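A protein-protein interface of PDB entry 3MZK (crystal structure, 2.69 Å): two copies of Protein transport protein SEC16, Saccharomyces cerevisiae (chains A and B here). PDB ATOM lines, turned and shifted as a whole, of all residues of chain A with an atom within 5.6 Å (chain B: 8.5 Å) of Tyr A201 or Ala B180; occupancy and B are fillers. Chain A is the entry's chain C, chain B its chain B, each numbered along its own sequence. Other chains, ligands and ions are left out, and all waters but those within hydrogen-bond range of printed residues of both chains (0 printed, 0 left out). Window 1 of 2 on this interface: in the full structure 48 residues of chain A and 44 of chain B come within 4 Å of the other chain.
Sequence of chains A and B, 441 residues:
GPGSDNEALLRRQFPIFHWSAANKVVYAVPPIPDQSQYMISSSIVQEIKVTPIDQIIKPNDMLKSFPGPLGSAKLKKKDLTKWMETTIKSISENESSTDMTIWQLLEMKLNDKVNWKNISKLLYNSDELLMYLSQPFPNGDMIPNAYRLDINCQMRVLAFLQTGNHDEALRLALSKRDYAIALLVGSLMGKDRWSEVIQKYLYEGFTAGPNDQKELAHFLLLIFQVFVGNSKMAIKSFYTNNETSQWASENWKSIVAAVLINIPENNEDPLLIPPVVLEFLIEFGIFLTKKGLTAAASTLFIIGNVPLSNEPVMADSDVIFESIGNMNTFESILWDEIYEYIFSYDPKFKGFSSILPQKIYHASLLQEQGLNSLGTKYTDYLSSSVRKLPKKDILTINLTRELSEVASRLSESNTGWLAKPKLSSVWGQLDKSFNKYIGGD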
ATOM      1  N   TYR A 179     -26.763  25.527  -3.917  1.00  0.00           N
ATOM      2  CA  TYR A 179     -25.642  25.286  -4.813  1.00  0.00           C
ATOM      3  C   TYR A 179     -25.154  23.843  -4.789  1.00  0.00           C
ATOM      4  O   TYR A 179     -24.368  23.438  -5.641  1.00  0.00           O
ATOM      5  CB  TYR A 179     -24.496  26.261  -4.518  1.00  0.00           C
ATOM      6  CG  TYR A 179     -24.900  27.714  -4.631  1.00  0.00           C
ATOM      7  CD1 TYR A 179     -25.092  28.309  -5.873  1.00  0.00           C
ATOM      8  CD2 TYR A 179     -25.094  28.493  -3.495  1.00  0.00           C
ATOM      9  CE1 TYR A 179     -25.465  29.640  -5.979  1.00  0.00           C
ATOM     10  CE2 TYR A 179     -25.467  29.824  -3.593  1.00  0.00           C
ATOM     11  CZ  TYR A 179     -25.650  30.390  -4.835  1.00  0.00           C
ATOM     12  OH  TYR A 179     -26.020  31.710  -4.933  1.00  0.00           O
ATOM     13  N   ALA A 180     -25.622  23.067  -3.819  1.00  0.00           N
ATOM     14  CA  ALA A 180     -25.267  21.652  -3.753  1.00  0.00           C
ATOM     15  C   ALA A 180     -25.868  20.899  -4.937  1.00  0.00           C
ATOM     16  O   ALA A 180     -25.137  20.359  -5.769  1.00  0.00           O
ATOM     17  CB  ALA A 180     -25.722  21.039  -2.437  1.00  0.00           C
ATOM     18  N   LEU A 183     -24.706  22.059  -8.297  1.00  0.00           N
ATOM     19  CA  LEU A 183     -23.481  21.388  -8.718  1.00  0.00           C
ATOM     20  C   LEU A 183     -23.768  19.987  -9.268  1.00  0.00           C
ATOM     21  O   LEU A 183     -23.276  19.613 -10.334  1.00  0.00           O
ATOM     22  CB  LEU A 183     -22.481  21.317  -7.559  1.00  0.00           C
ATOM     23  CG  LEU A 183     -21.777  22.635  -7.212  1.00  0.00           C
ATOM     24  CD1 LEU A 183     -20.843  22.478  -6.012  1.00  0.00           C
ATOM     25  CD2 LEU A 183     -21.009  23.152  -8.415  1.00  0.00           C
ATOM     26  N   GLU A 196     -20.069  27.676 -14.168  1.00  0.00           N
ATOM     27  CA  GLU A 196     -20.947  28.806 -13.873  1.00  0.00           C
ATOM     28  C   GLU A 196     -21.541  28.692 -12.472  1.00  0.00           C
ATOM     29  O   GLU A 196     -21.700  29.695 -11.769  1.00  0.00           O
ATOM     30  CB  GLU A 196     -22.062  28.918 -14.915  1.00  0.00           C
ATOM     31  N   VAL A 197     -21.861  27.465 -12.068  1.00  0.00           N
ATOM     32  CA  VAL A 197     -22.397  27.221 -10.734  1.00  0.00           C
ATOM     33  C   VAL A 197     -21.354  27.555  -9.672  1.00  0.00           C
ATOM     34  O   VAL A 197     -21.673  28.135  -8.634  1.00  0.00           O
ATOM     35  CB  VAL A 197     -22.853  25.766 -10.555  1.00  0.00           C
ATOM     36  CG1 VAL A 197     -23.338  25.546  -9.132  1.00  0.00           C
ATOM     37  CG2 VAL A 197     -23.952  25.415 -11.563  1.00  0.00           C
ATOM     38  N   ILE A 198     -20.105  27.190  -9.939  1.00  0.00           N
ATOM     39  CA  ILE A 198     -19.016  27.485  -9.017  1.00  0.00           C
ATOM     40  C   ILE A 198     -18.910  28.988  -8.772  1.00  0.00           C
ATOM     41  O   ILE A 198     -18.774  29.442  -7.631  1.00  0.00           O
ATOM     42  CB  ILE A 198     -17.670  26.974  -9.554  1.00  0.00           C
ATOM     43  CG1 ILE A 198     -17.754  25.478  -9.871  1.00  0.00           C
ATOM     44  CG2 ILE A 198     -16.567  27.243  -8.550  1.00  0.00           C
ATOM     45  CD1 ILE A 198     -16.456  24.885 -10.363  1.00  0.00           C
ATOM     46  N   GLN A 199     -18.976  29.757  -9.854  1.00  0.00           N
ATOM     47  CA  GLN A 199     -18.885  31.206  -9.761  1.00  0.00           C
ATOM     48  C   GLN A 199     -20.018  31.762  -8.911  1.00  0.00           C
ATOM     49  O   GLN A 199     -19.784  32.559  -8.002  1.00  0.00           O
ATOM     50  CB  GLN A 199     -18.906  31.841 -11.150  1.00  0.00           C
ATOM     51  CG  GLN A 199     -17.860  31.280 -12.093  1.00  0.00           C
ATOM     52  CD  GLN A 199     -17.549  32.214 -13.243  1.00  0.00           C
ATOM     53  OE1 GLN A 199     -17.908  33.393 -13.215  1.00  0.00           O
ATOM     54  NE2 GLN A 199     -16.874  31.694 -14.262  1.00  0.00           N
ATOM     55  N   LYS A 200     -21.242  31.333  -9.206  1.00  0.00           N
ATOM     56  CA  LYS A 200     -22.412  31.855  -8.511  1.00  0.00           C
ATOM     57  C   LYS A 200     -22.341  31.539  -7.019  1.00  0.00           C
ATOM     58  O   LYS A 200     -22.688  32.370  -6.180  1.00  0.00           O
ATOM     59  CB  LYS A 200     -23.709  31.322  -9.134  1.00  0.00           C
ATOM     60  N   TYR A 201     -21.864  30.346  -6.688  1.00  0.00           N
ATOM     61  CA  TYR A 201     -21.750  29.955  -5.290  1.00  0.00           C
ATOM     62  C   TYR A 201     -20.731  30.826  -4.552  1.00  0.00           C
ATOM     63  O   TYR A 201     -20.995  31.305  -3.449  1.00  0.00           O
ATOM     64  CB  TYR A 201     -21.403  28.468  -5.162  1.00  0.00           C
ATOM     65  CG  TYR A 201     -20.850  28.099  -3.807  1.00  0.00           C
ATOM     66  CD1 TYR A 201     -21.679  28.008  -2.694  1.00  0.00           C
ATOM     67  CD2 TYR A 201     -19.494  27.855  -3.637  1.00  0.00           C
ATOM     68  CE1 TYR A 201     -21.168  27.682  -1.456  1.00  0.00           C
ATOM     69  CE2 TYR A 201     -18.979  27.530  -2.408  1.00  0.00           C
ATOM     70  CZ  TYR A 201     -19.816  27.444  -1.322  1.00  0.00           C
ATOM     71  OH  TYR A 201     -19.295  27.121  -0.096  1.00  0.00           O
ATOM     72  N   LEU A 202     -19.576  31.044  -5.173  1.00  0.00           N
ATOM     73  CA  LEU A 202     -18.515  31.827  -4.550  1.00  0.00           C
ATOM     74  C   LEU A 202     -18.843  33.317  -4.463  1.00  0.00           C
ATOM     75  O   LEU A 202     -18.653  33.939  -3.419  1.00  0.00           O
ATOM     76  CB  LEU A 202     -17.199  31.633  -5.305  1.00  0.00           C
ATOM     77  CG  LEU A 202     -16.584  30.233  -5.285  1.00  0.00           C
ATOM     78  CD1 LEU A 202     -15.359  30.177  -6.183  1.00  0.00           C
ATOM     79  CD2 LEU A 202     -16.224  29.825  -3.869  1.00  0.00           C
ATOM     80  N   TYR A 203     -19.341  33.880  -5.561  1.00  0.00           N
ATOM     81  CA  TYR A 203     -19.486  35.328  -5.689  1.00  0.00           C
ATOM     82  C   TYR A 203     -20.867  35.867  -5.321  1.00  0.00           C
ATOM     83  O   TYR A 203     -21.061  37.079  -5.241  1.00  0.00           O
ATOM     84  CB  TYR A 203     -19.107  35.772  -7.105  1.00  0.00           C
ATOM     85  CG  TYR A 203     -17.632  35.627  -7.413  1.00  0.00           C
ATOM     86  CD1 TYR A 203     -16.747  36.666  -7.160  1.00  0.00           C
ATOM     87  CD2 TYR A 203     -17.123  34.451  -7.951  1.00  0.00           C
ATOM     88  CE1 TYR A 203     -15.397  36.542  -7.437  1.00  0.00           C
ATOM     89  CE2 TYR A 203     -15.772  34.319  -8.229  1.00  0.00           C
ATOM     90  CZ  TYR A 203     -14.916  35.369  -7.970  1.00  0.00           C
ATOM     91  OH  TYR A 203     -13.571  35.256  -8.242  1.00  0.00           O
ATOM     92  N   GLU A 204     -21.825  34.974  -5.094  1.00  0.00           N
ATOM     93  CA  GLU A 204     -23.173  35.397  -4.728  1.00  0.00           C
ATOM     94  C   GLU A 204     -23.145  36.308  -3.500  1.00  0.00           C
ATOM     95  O   GLU A 204     -23.851  37.315  -3.445  1.00  0.00           O
ATOM     96  CB  GLU A 204     -24.071  34.186  -4.468  1.00  0.00           C
ATOM     97  N   GLY A 205     -22.317  35.950  -2.525  1.00  0.00           N
ATOM     98  CA  GLY A 205     -22.184  36.731  -1.309  1.00  0.00           C
ATOM     99  C   GLY A 205     -21.650  35.902  -0.159  1.00  0.00           C
ATOM    100  O   GLY A 205     -21.551  34.680  -0.261  1.00  0.00           O
ATOM    101  N   TYR B 147     -26.423  25.294   5.598  1.00  0.00           N
ATOM    102  CA  TYR B 147     -25.200  25.868   6.134  1.00  0.00           C
ATOM    103  C   TYR B 147     -24.183  26.201   5.055  1.00  0.00           C
ATOM    104  O   TYR B 147     -24.235  25.678   3.944  1.00  0.00           O
ATOM    105  CB  TYR B 147     -24.610  24.960   7.209  1.00  0.00           C
ATOM    106  CG  TYR B 147     -25.557  24.798   8.368  1.00  0.00           C
ATOM    107  CD1 TYR B 147     -25.482  25.637   9.470  1.00  0.00           C
ATOM    108  CD2 TYR B 147     -26.554  23.834   8.344  1.00  0.00           C
ATOM    109  CE1 TYR B 147     -26.356  25.504  10.527  1.00  0.00           C
ATOM    110  CE2 TYR B 147     -27.434  23.692   9.397  1.00  0.00           C
ATOM    111  CZ  TYR B 147     -27.330  24.530  10.488  1.00  0.00           C
ATOM    112  OH  TYR B 147     -28.204  24.396  11.543  1.00  0.00           O
ATOM    113  N   ARG B 148     -23.264  27.089   5.406  1.00  0.00           N
ATOM    114  CA  ARG B 148     -22.305  27.638   4.467  1.00  0.00           C
ATOM    115  C   ARG B 148     -21.095  28.145   5.238  1.00  0.00           C
ATOM    116  O   ARG B 148     -21.240  28.803   6.266  1.00  0.00           O
ATOM    117  CB  ARG B 148     -22.948  28.787   3.700  1.00  0.00           C
ATOM    118  CG  ARG B 148     -22.009  29.536   2.791  1.00  0.00           C
ATOM    119  CD  ARG B 148     -22.666  30.786   2.252  1.00  0.00           C
ATOM    120  NE  ARG B 148     -21.848  31.391   1.209  1.00  0.00           N
ATOM    121  CZ  ARG B 148     -22.051  31.216  -0.092  1.00  0.00           C
ATOM    122  NH1 ARG B 148     -23.055  30.464  -0.510  1.00  0.00           N
ATOM    123  NH2 ARG B 148     -21.254  31.803  -0.973  1.00  0.00           N
ATOM    124  N   LEU B 149     -19.905  27.831   4.743  1.00  0.00           N
ATOM    125  CA  LEU B 149     -18.668  28.248   5.398  1.00  0.00           C
ATOM    126  C   LEU B 149     -18.561  29.764   5.527  1.00  0.00           C
ATOM    127  O   LEU B 149     -18.813  30.495   4.573  1.00  0.00           O
ATOM    128  CB  LEU B 149     -17.457  27.704   4.637  1.00  0.00           C
ATOM    129  CG  LEU B 149     -16.809  26.443   5.203  1.00  0.00           C
ATOM    130  CD1 LEU B 149     -17.837  25.354   5.472  1.00  0.00           C
ATOM    131  CD2 LEU B 149     -15.725  25.953   4.271  1.00  0.00           C
ATOM    132  N   ASP B 150     -18.193  30.231   6.717  1.00  0.00           N
ATOM    133  CA  ASP B 150     -17.926  31.651   6.937  1.00  0.00           C
ATOM    134  C   ASP B 150     -16.527  32.011   6.445  1.00  0.00           C
ATOM    135  O   ASP B 150     -15.789  31.143   5.977  1.00  0.00           O
ATOM    136  CB  ASP B 150     -18.086  32.027   8.417  1.00  0.00           C
ATOM    137  CG  ASP B 150     -17.170  31.227   9.336  1.00  0.00           C
ATOM    138  OD1 ASP B 150     -16.228  30.572   8.841  1.00  0.00           O
ATOM    139  OD2 ASP B 150     -17.392  31.260  10.565  1.00  0.00           O
ATOM    140  N   GLN B 154     -13.698  29.385   5.401  1.00  0.00           N
ATOM    141  CA  GLN B 154     -13.379  29.524   3.990  1.00  0.00           C
ATOM    142  C   GLN B 154     -11.874  29.688   3.788  1.00  0.00           C
ATOM    143  O   GLN B 154     -11.293  29.083   2.890  1.00  0.00           O
ATOM    144  CB  GLN B 154     -14.141  30.701   3.390  1.00  0.00           C
ATOM    145  CG  GLN B 154     -14.257  30.667   1.884  1.00  0.00           C
ATOM    146  CD  GLN B 154     -15.101  31.803   1.364  1.00  0.00           C
ATOM    147  OE1 GLN B 154     -15.596  32.622   2.139  1.00  0.00           O
ATOM    148  NE2 GLN B 154     -15.275  31.860   0.049  1.00  0.00           N
ATOM    149  N   VAL B 157     -10.076  26.282   4.442  1.00  0.00           N
ATOM    150  CA  VAL B 157     -10.189  25.392   3.294  1.00  0.00           C
ATOM    151  C   VAL B 157      -9.175  25.743   2.210  1.00  0.00           C
ATOM    152  O   VAL B 157      -8.532  24.862   1.640  1.00  0.00           O
ATOM    153  CB  VAL B 157     -11.603  25.429   2.693  1.00  0.00           C
ATOM    154  CG1 VAL B 157     -11.648  24.637   1.403  1.00  0.00           C
ATOM    155  CG2 VAL B 157     -12.606  24.883   3.690  1.00  0.00           C
ATOM    156  N   LEU B 170     -11.946  18.403   3.125  1.00  0.00           N
ATOM    157  CA  LEU B 170     -13.265  17.789   3.043  1.00  0.00           C
ATOM    158  C   LEU B 170     -13.883  17.589   4.423  1.00  0.00           C
ATOM    159  O   LEU B 170     -15.066  17.869   4.630  1.00  0.00           O
ATOM    160  CB  LEU B 170     -13.183  16.451   2.314  1.00  0.00           C
ATOM    161  CG  LEU B 170     -14.504  15.693   2.181  1.00  0.00           C
ATOM    162  CD1 LEU B 170     -15.524  16.540   1.444  1.00  0.00           C
ATOM    163  CD2 LEU B 170     -14.293  14.360   1.473  1.00  0.00           C
ATOM    164  N   ALA B 173     -15.329  20.803   5.612  1.00  0.00           N
ATOM    165  CA  ALA B 173     -16.520  21.226   4.883  1.00  0.00           C
ATOM    166  C   ALA B 173     -17.741  20.415   5.295  1.00  0.00           C
ATOM    167  O   ALA B 173     -18.856  20.933   5.341  1.00  0.00           O
ATOM    168  CB  ALA B 173     -16.294  21.119   3.386  1.00  0.00           C
ATOM    169  N   LEU B 174     -17.523  19.140   5.594  1.00  0.00           N
ATOM    170  CA  LEU B 174     -18.613  18.266   6.009  1.00  0.00           C
ATOM    171  C   LEU B 174     -19.041  18.535   7.453  1.00  0.00           C
ATOM    172  O   LEU B 174     -20.223  18.437   7.784  1.00  0.00           O
ATOM    173  CB  LEU B 174     -18.227  16.795   5.835  1.00  0.00           C
ATOM    174  CG  LEU B 174     -18.090  16.267   4.407  1.00  0.00           C
ATOM    175  CD1 LEU B 174     -17.719  14.790   4.432  1.00  0.00           C
ATOM    176  CD2 LEU B 174     -19.375  16.481   3.634  1.00  0.00           C
ATOM    177  N   ARG B 177     -21.266  21.240   7.507  1.00  0.00           N
ATOM    178  CA  ARG B 177     -22.432  20.936   6.685  1.00  0.00           C
ATOM    179  C   ARG B 177     -22.549  21.815   5.446  1.00  0.00           C
ATOM    180  O   ARG B 177     -23.650  22.115   4.996  1.00  0.00           O
ATOM    181  CB  ARG B 177     -23.721  21.011   7.511  1.00  0.00           C
ATOM    182  CG  ARG B 177     -23.759  20.062   8.703  1.00  0.00           C
ATOM    183  CD  ARG B 177     -25.183  19.872   9.211  1.00  0.00           C
ATOM    184  NE  ARG B 177     -26.022  19.225   8.203  1.00  0.00           N
ATOM    185  CZ  ARG B 177     -27.317  18.961   8.353  1.00  0.00           C
ATOM    186  NH1 ARG B 177     -27.937  19.290   9.477  1.00  0.00           N
ATOM    187  NH2 ARG B 177     -27.991  18.370   7.375  1.00  0.00           N
ATOM    188  N   ASP B 178     -21.413  22.220   4.892  1.00  0.00           N
ATOM    189  CA  ASP B 178     -21.413  22.974   3.642  1.00  0.00           C
ATOM    190  C   ASP B 178     -21.150  22.029   2.482  1.00  0.00           C
ATOM    191  O   ASP B 178     -20.006  21.794   2.101  1.00  0.00           O
ATOM    192  CB  ASP B 178     -20.359  24.078   3.665  1.00  0.00           C
ATOM    193  CG  ASP B 178     -20.475  25.013   2.480  1.00  0.00           C
ATOM    194  OD1 ASP B 178     -20.926  24.565   1.403  1.00  0.00           O
ATOM    195  OD2 ASP B 178     -20.120  26.201   2.626  1.00  0.00           O
ATOM    196  N   TYR B 179     -22.223  21.493   1.917  1.00  0.00           N
ATOM    197  CA  TYR B 179     -22.104  20.418   0.943  1.00  0.00           C
ATOM    198  C   TYR B 179     -21.695  20.908  -0.440  1.00  0.00           C
ATOM    199  O   TYR B 179     -21.344  20.110  -1.306  1.00  0.00           O
ATOM    200  CB  TYR B 179     -23.399  19.607   0.881  1.00  0.00           C
ATOM    201  CG  TYR B 179     -23.788  19.005   2.215  1.00  0.00           C
ATOM    202  CD1 TYR B 179     -23.108  17.909   2.729  1.00  0.00           C
ATOM    203  CD2 TYR B 179     -24.832  19.536   2.961  1.00  0.00           C
ATOM    204  CE1 TYR B 179     -23.459  17.357   3.951  1.00  0.00           C
ATOM    205  CE2 TYR B 179     -25.189  18.993   4.181  1.00  0.00           C
ATOM    206  CZ  TYR B 179     -24.500  17.904   4.671  1.00  0.00           C
ATOM    207  OH  TYR B 179     -24.853  17.361   5.885  1.00  0.00           O
ATOM    208  N   ALA B 180     -21.733  22.218  -0.644  1.00  0.00           N
ATOM    209  CA  ALA B 180     -21.313  22.787  -1.914  1.00  0.00           C
ATOM    210  C   ALA B 180     -19.810  22.605  -2.101  1.00  0.00           C
ATOM    211  O   ALA B 180     -19.374  21.949  -3.042  1.00  0.00           O
ATOM    212  CB  ALA B 180     -21.697  24.259  -1.998  1.00  0.00           C
ATOM    213  N   ILE B 181     -19.022  23.182  -1.197  1.00  0.00           N
ATOM    214  CA  ILE B 181     -17.569  23.050  -1.264  1.00  0.00           C
ATOM    215  C   ILE B 181     -17.172  21.611  -1.029  1.00  0.00           C
ATOM    216  O   ILE B 181     -16.151  21.152  -1.535  1.00  0.00           O
ATOM    217  CB  ILE B 181     -16.856  23.910  -0.205  1.00  0.00           C
ATOM    218  CG1 ILE B 181     -17.876  24.687   0.615  1.00  0.00           C
ATOM    219  CG2 ILE B 181     -15.837  24.851  -0.851  1.00  0.00           C
ATOM    220  CD1 ILE B 181     -17.250  25.685   1.531  1.00  0.00           C
ATOM    221  N   ALA B 182     -17.973  20.904  -0.242  1.00  0.00           N
ATOM    222  CA  ALA B 182     -17.713  19.496  -0.004  1.00  0.00           C
ATOM    223  C   ALA B 182     -17.671  18.790  -1.354  1.00  0.00           C
ATOM    224  O   ALA B 182     -16.739  18.042  -1.645  1.00  0.00           O
ATOM    225  CB  ALA B 182     -18.779  18.900   0.892  1.00  0.00           C
ATOM    226  N   LEU B 183     -18.675  19.057  -2.187  1.00  0.00           N
ATOM    227  CA  LEU B 183     -18.739  18.489  -3.530  1.00  0.00           C
ATOM    228  C   LEU B 183     -17.536  18.912  -4.368  1.00  0.00           C
ATOM    229  O   LEU B 183     -16.893  18.081  -5.016  1.00  0.00           O
ATOM    230  CB  LEU B 183     -20.051  18.876  -4.230  1.00  0.00           C
ATOM    231  CG  LEU B 183     -21.296  18.134  -3.736  1.00  0.00           C
ATOM    232  CD1 LEU B 183     -22.559  18.626  -4.431  1.00  0.00           C
ATOM    233  CD2 LEU B 183     -21.128  16.627  -3.922  1.00  0.00           C
ATOM    234  N   LEU B 184     -17.235  20.205  -4.348  1.00  0.00           N
ATOM    235  CA  LEU B 184     -16.085  20.737  -5.066  1.00  0.00           C
ATOM    236  C   LEU B 184     -14.789  20.043  -4.650  1.00  0.00           C
ATOM    237  O   LEU B 184     -14.089  19.471  -5.483  1.00  0.00           O
ATOM    238  CB  LEU B 184     -15.976  22.242  -4.849  1.00  0.00           C
ATOM    239  CG  LEU B 184     -17.175  22.996  -5.413  1.00  0.00           C
ATOM    240  CD1 LEU B 184     -17.095  24.486  -5.094  1.00  0.00           C
ATOM    241  CD2 LEU B 184     -17.270  22.756  -6.912  1.00  0.00           C
ATOM    242  N   VAL B 185     -14.471  20.091  -3.361  1.00  0.00           N
ATOM    243  CA  VAL B 185     -13.274  19.428  -2.864  1.00  0.00           C
ATOM    244  C   VAL B 185     -13.309  17.953  -3.246  1.00  0.00           C
ATOM    245  O   VAL B 185     -12.315  17.393  -3.707  1.00  0.00           O
ATOM    246  CB  VAL B 185     -13.131  19.572  -1.337  1.00  0.00           C
ATOM    247  CG1 VAL B 185     -12.014  18.685  -0.823  1.00  0.00           C
ATOM    248  CG2 VAL B 185     -12.877  21.023  -0.964  1.00  0.00           C
ATOM    249  N   GLY B 186     -14.471  17.334  -3.067  1.00  0.00           N
ATOM    250  CA  GLY B 186     -14.653  15.933  -3.394  1.00  0.00           C
ATOM    251  C   GLY B 186     -14.310  15.591  -4.830  1.00  0.00           C
ATOM    252  O   GLY B 186     -13.848  14.489  -5.111  1.00  0.00           O
ATOM    253  N   SER B 187     -14.531  16.528  -5.745  1.00  0.00           N
ATOM    254  CA  SER B 187     -14.250  16.276  -7.154  1.00  0.00           C
ATOM    255  C   SER B 187     -12.746  16.166  -7.419  1.00  0.00           C
ATOM    256  O   SER B 187     -12.324  15.544  -8.390  1.00  0.00           O
ATOM    257  CB  SER B 187     -14.890  17.348  -8.042  1.00  0.00           C
ATOM    258  OG  SER B 187     -14.283  18.617  -7.860  1.00  0.00           O
ATOM    259  N   TRP B 194     -16.666  11.669  -3.693  1.00  0.00           N
ATOM    260  CA  TRP B 194     -17.719  12.440  -4.339  1.00  0.00           C
ATOM    261  C   TRP B 194     -19.076  11.843  -3.983  1.00  0.00           C
ATOM    262  O   TRP B 194     -19.989  12.546  -3.551  1.00  0.00           O
ATOM    263  CB  TRP B 194     -17.526  12.436  -5.856  1.00  0.00           C
ATOM    264  CG  TRP B 194     -18.682  13.012  -6.615  1.00  0.00           C
ATOM    265  CD1 TRP B 194     -19.748  12.328  -7.129  1.00  0.00           C
ATOM    266  CD2 TRP B 194     -18.889  14.388  -6.949  1.00  0.00           C
ATOM    267  NE1 TRP B 194     -20.607  13.196  -7.762  1.00  0.00           N
ATOM    268  CE2 TRP B 194     -20.101  14.467  -7.665  1.00  0.00           C
ATOM    269  CE3 TRP B 194     -18.170  15.562  -6.710  1.00  0.00           C
ATOM    270  CZ2 TRP B 194     -20.607  15.671  -8.146  1.00  0.00           C
ATOM    271  CZ3 TRP B 194     -18.675  16.757  -7.187  1.00  0.00           C
ATOM    272  CH2 TRP B 194     -19.882  16.802  -7.896  1.00  0.00           C
ATOM    273  N   VAL B 197     -20.205  12.274  -0.338  1.00  0.00           N
ATOM    274  CA  VAL B 197     -20.721  13.612  -0.091  1.00  0.00           C
ATOM    275  C   VAL B 197     -22.183  13.699  -0.516  1.00  0.00           C
ATOM    276  O   VAL B 197     -23.001  14.318   0.167  1.00  0.00           O
ATOM    277  CB  VAL B 197     -19.899  14.685  -0.833  1.00  0.00           C
ATOM    278  CG1 VAL B 197     -20.513  16.068  -0.629  1.00  0.00           C
ATOM    279  CG2 VAL B 197     -18.447  14.663  -0.364  1.00  0.00           C
ATOM    280  N   TYR B 201     -25.272  14.745   1.980  1.00  0.00           N
ATOM    281  CA  TYR B 201     -26.122  15.893   1.669  1.00  0.00           C
ATOM    282  C   TYR B 201     -27.603  15.505   1.633  1.00  0.00           C
ATOM    283  O   TYR B 201     -28.449  16.192   2.203  1.00  0.00           O
ATOM    284  CB  TYR B 201     -25.698  16.557   0.350  1.00  0.00           C
ATOM    285  CG  TYR B 201     -26.762  17.445  -0.243  1.00  0.00           C
ATOM    286  CD1 TYR B 201     -27.035  18.694   0.299  1.00  0.00           C
ATOM    287  CD2 TYR B 201     -27.504  17.028  -1.337  1.00  0.00           C
ATOM    288  CE1 TYR B 201     -28.017  19.507  -0.237  1.00  0.00           C
ATOM    289  CE2 TYR B 201     -28.485  17.829  -1.880  1.00  0.00           C
ATOM    290  CZ  TYR B 201     -28.740  19.067  -1.326  1.00  0.00           C
ATOM    291  OH  TYR B 201     -29.724  19.862  -1.868  1.00  0.00           O
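The backbone carbonyl oxygen of Gly A205 sits at hydrogen-bond distance from the guanidinium group of Arg B148 (3.0 Å). The backbone carbonyl oxygen of Tyr A201 lies within hydrogen-bond range of the guanidinium group of Arg B148 (2.5 Å). The side-chain hydroxyl of Tyr A201 lies within hydrogen-bond range of the side-chain carboxylate of Asp B178.
The backbone carbonyl oxygen of Leu B184 is in hydrogen-bond range of the side-chain hydroxyl of Ser B187, 2.5 Å away. The side-chain carboxylate (OD1) of Asp B178 sits close to the backbone NH (N) of Ala B180. O of Ala B173 sits at hydrogen-bond distance from N of Asp B178 (2.9 Å). OD2 of Asp B178 lies within hydrogen-bond range of N of Leu B149 (2.7 Å).
Tyr A179 touches Arg B148 (CE2 to NH1, 3.97 Å). Ala A180 touches Leu B183 (O to CD1, 3.4 Å). Ala A180 touches Tyr B201. Ala B180 touches Leu A183 (O to CD1, 3.4 Å). CD1 of Leu A183 touches CD2 of Leu B184, at 3.7 Å. Ala B180 touches Tyr A201 (CB to CE1, 3.5 Å). Tyr A201 touches Ile B181.
Tyr A201 touches just these residues of chain B: Arg B148 (2.5 Å), Asp B178 (3.0 Å), Ala B180 (3.5 Å) and Ile B181 (2.9 Å). Ala B180 touches just these residues of chain A: Leu A183 (3.4 Å) and Tyr A201 (3.5 Å). Of the printed residues of chain A, Leu B183 touches Ala A180. Of the printed residues of chain B, Leu A183 touches Ala B180 and Leu B184. Tyr A203 touches none of the printed residues of chain B. The nearest residue of chain A that does not touch Ala B180 is Tyr A179 (4.3 Å).
Printed residues of chain A that touch a printed residue of chain B: Tyr A179, Ala A180, Leu A183, Tyr A201 and Gly A205. Of the 23 printed residues of chain B, 7 touch a printed residue of chain A. Hydrophobic or aromatic side chains of chain B within 4 Å of the printed part of chain A: Ala B180, Ile B181, Leu B183, Leu B184 and Tyr B201. Among the printed residues, no Asp or Glu carboxylate lies within 4 Å of a Lys or Arg side-chain nitrogen of the other chain.
Ala A180 touches Leu B183, and with the chains exchanged Leu A183 touches Ala B180. Ala A180 touches Tyr B201, and with the chains exchanged Tyr A201 touches Ala B180. 5 positions are printed for both chains. Of the 10 pairs that touch across the chains among the printed residues, 4 have their exchanged pair printed and touching as well.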
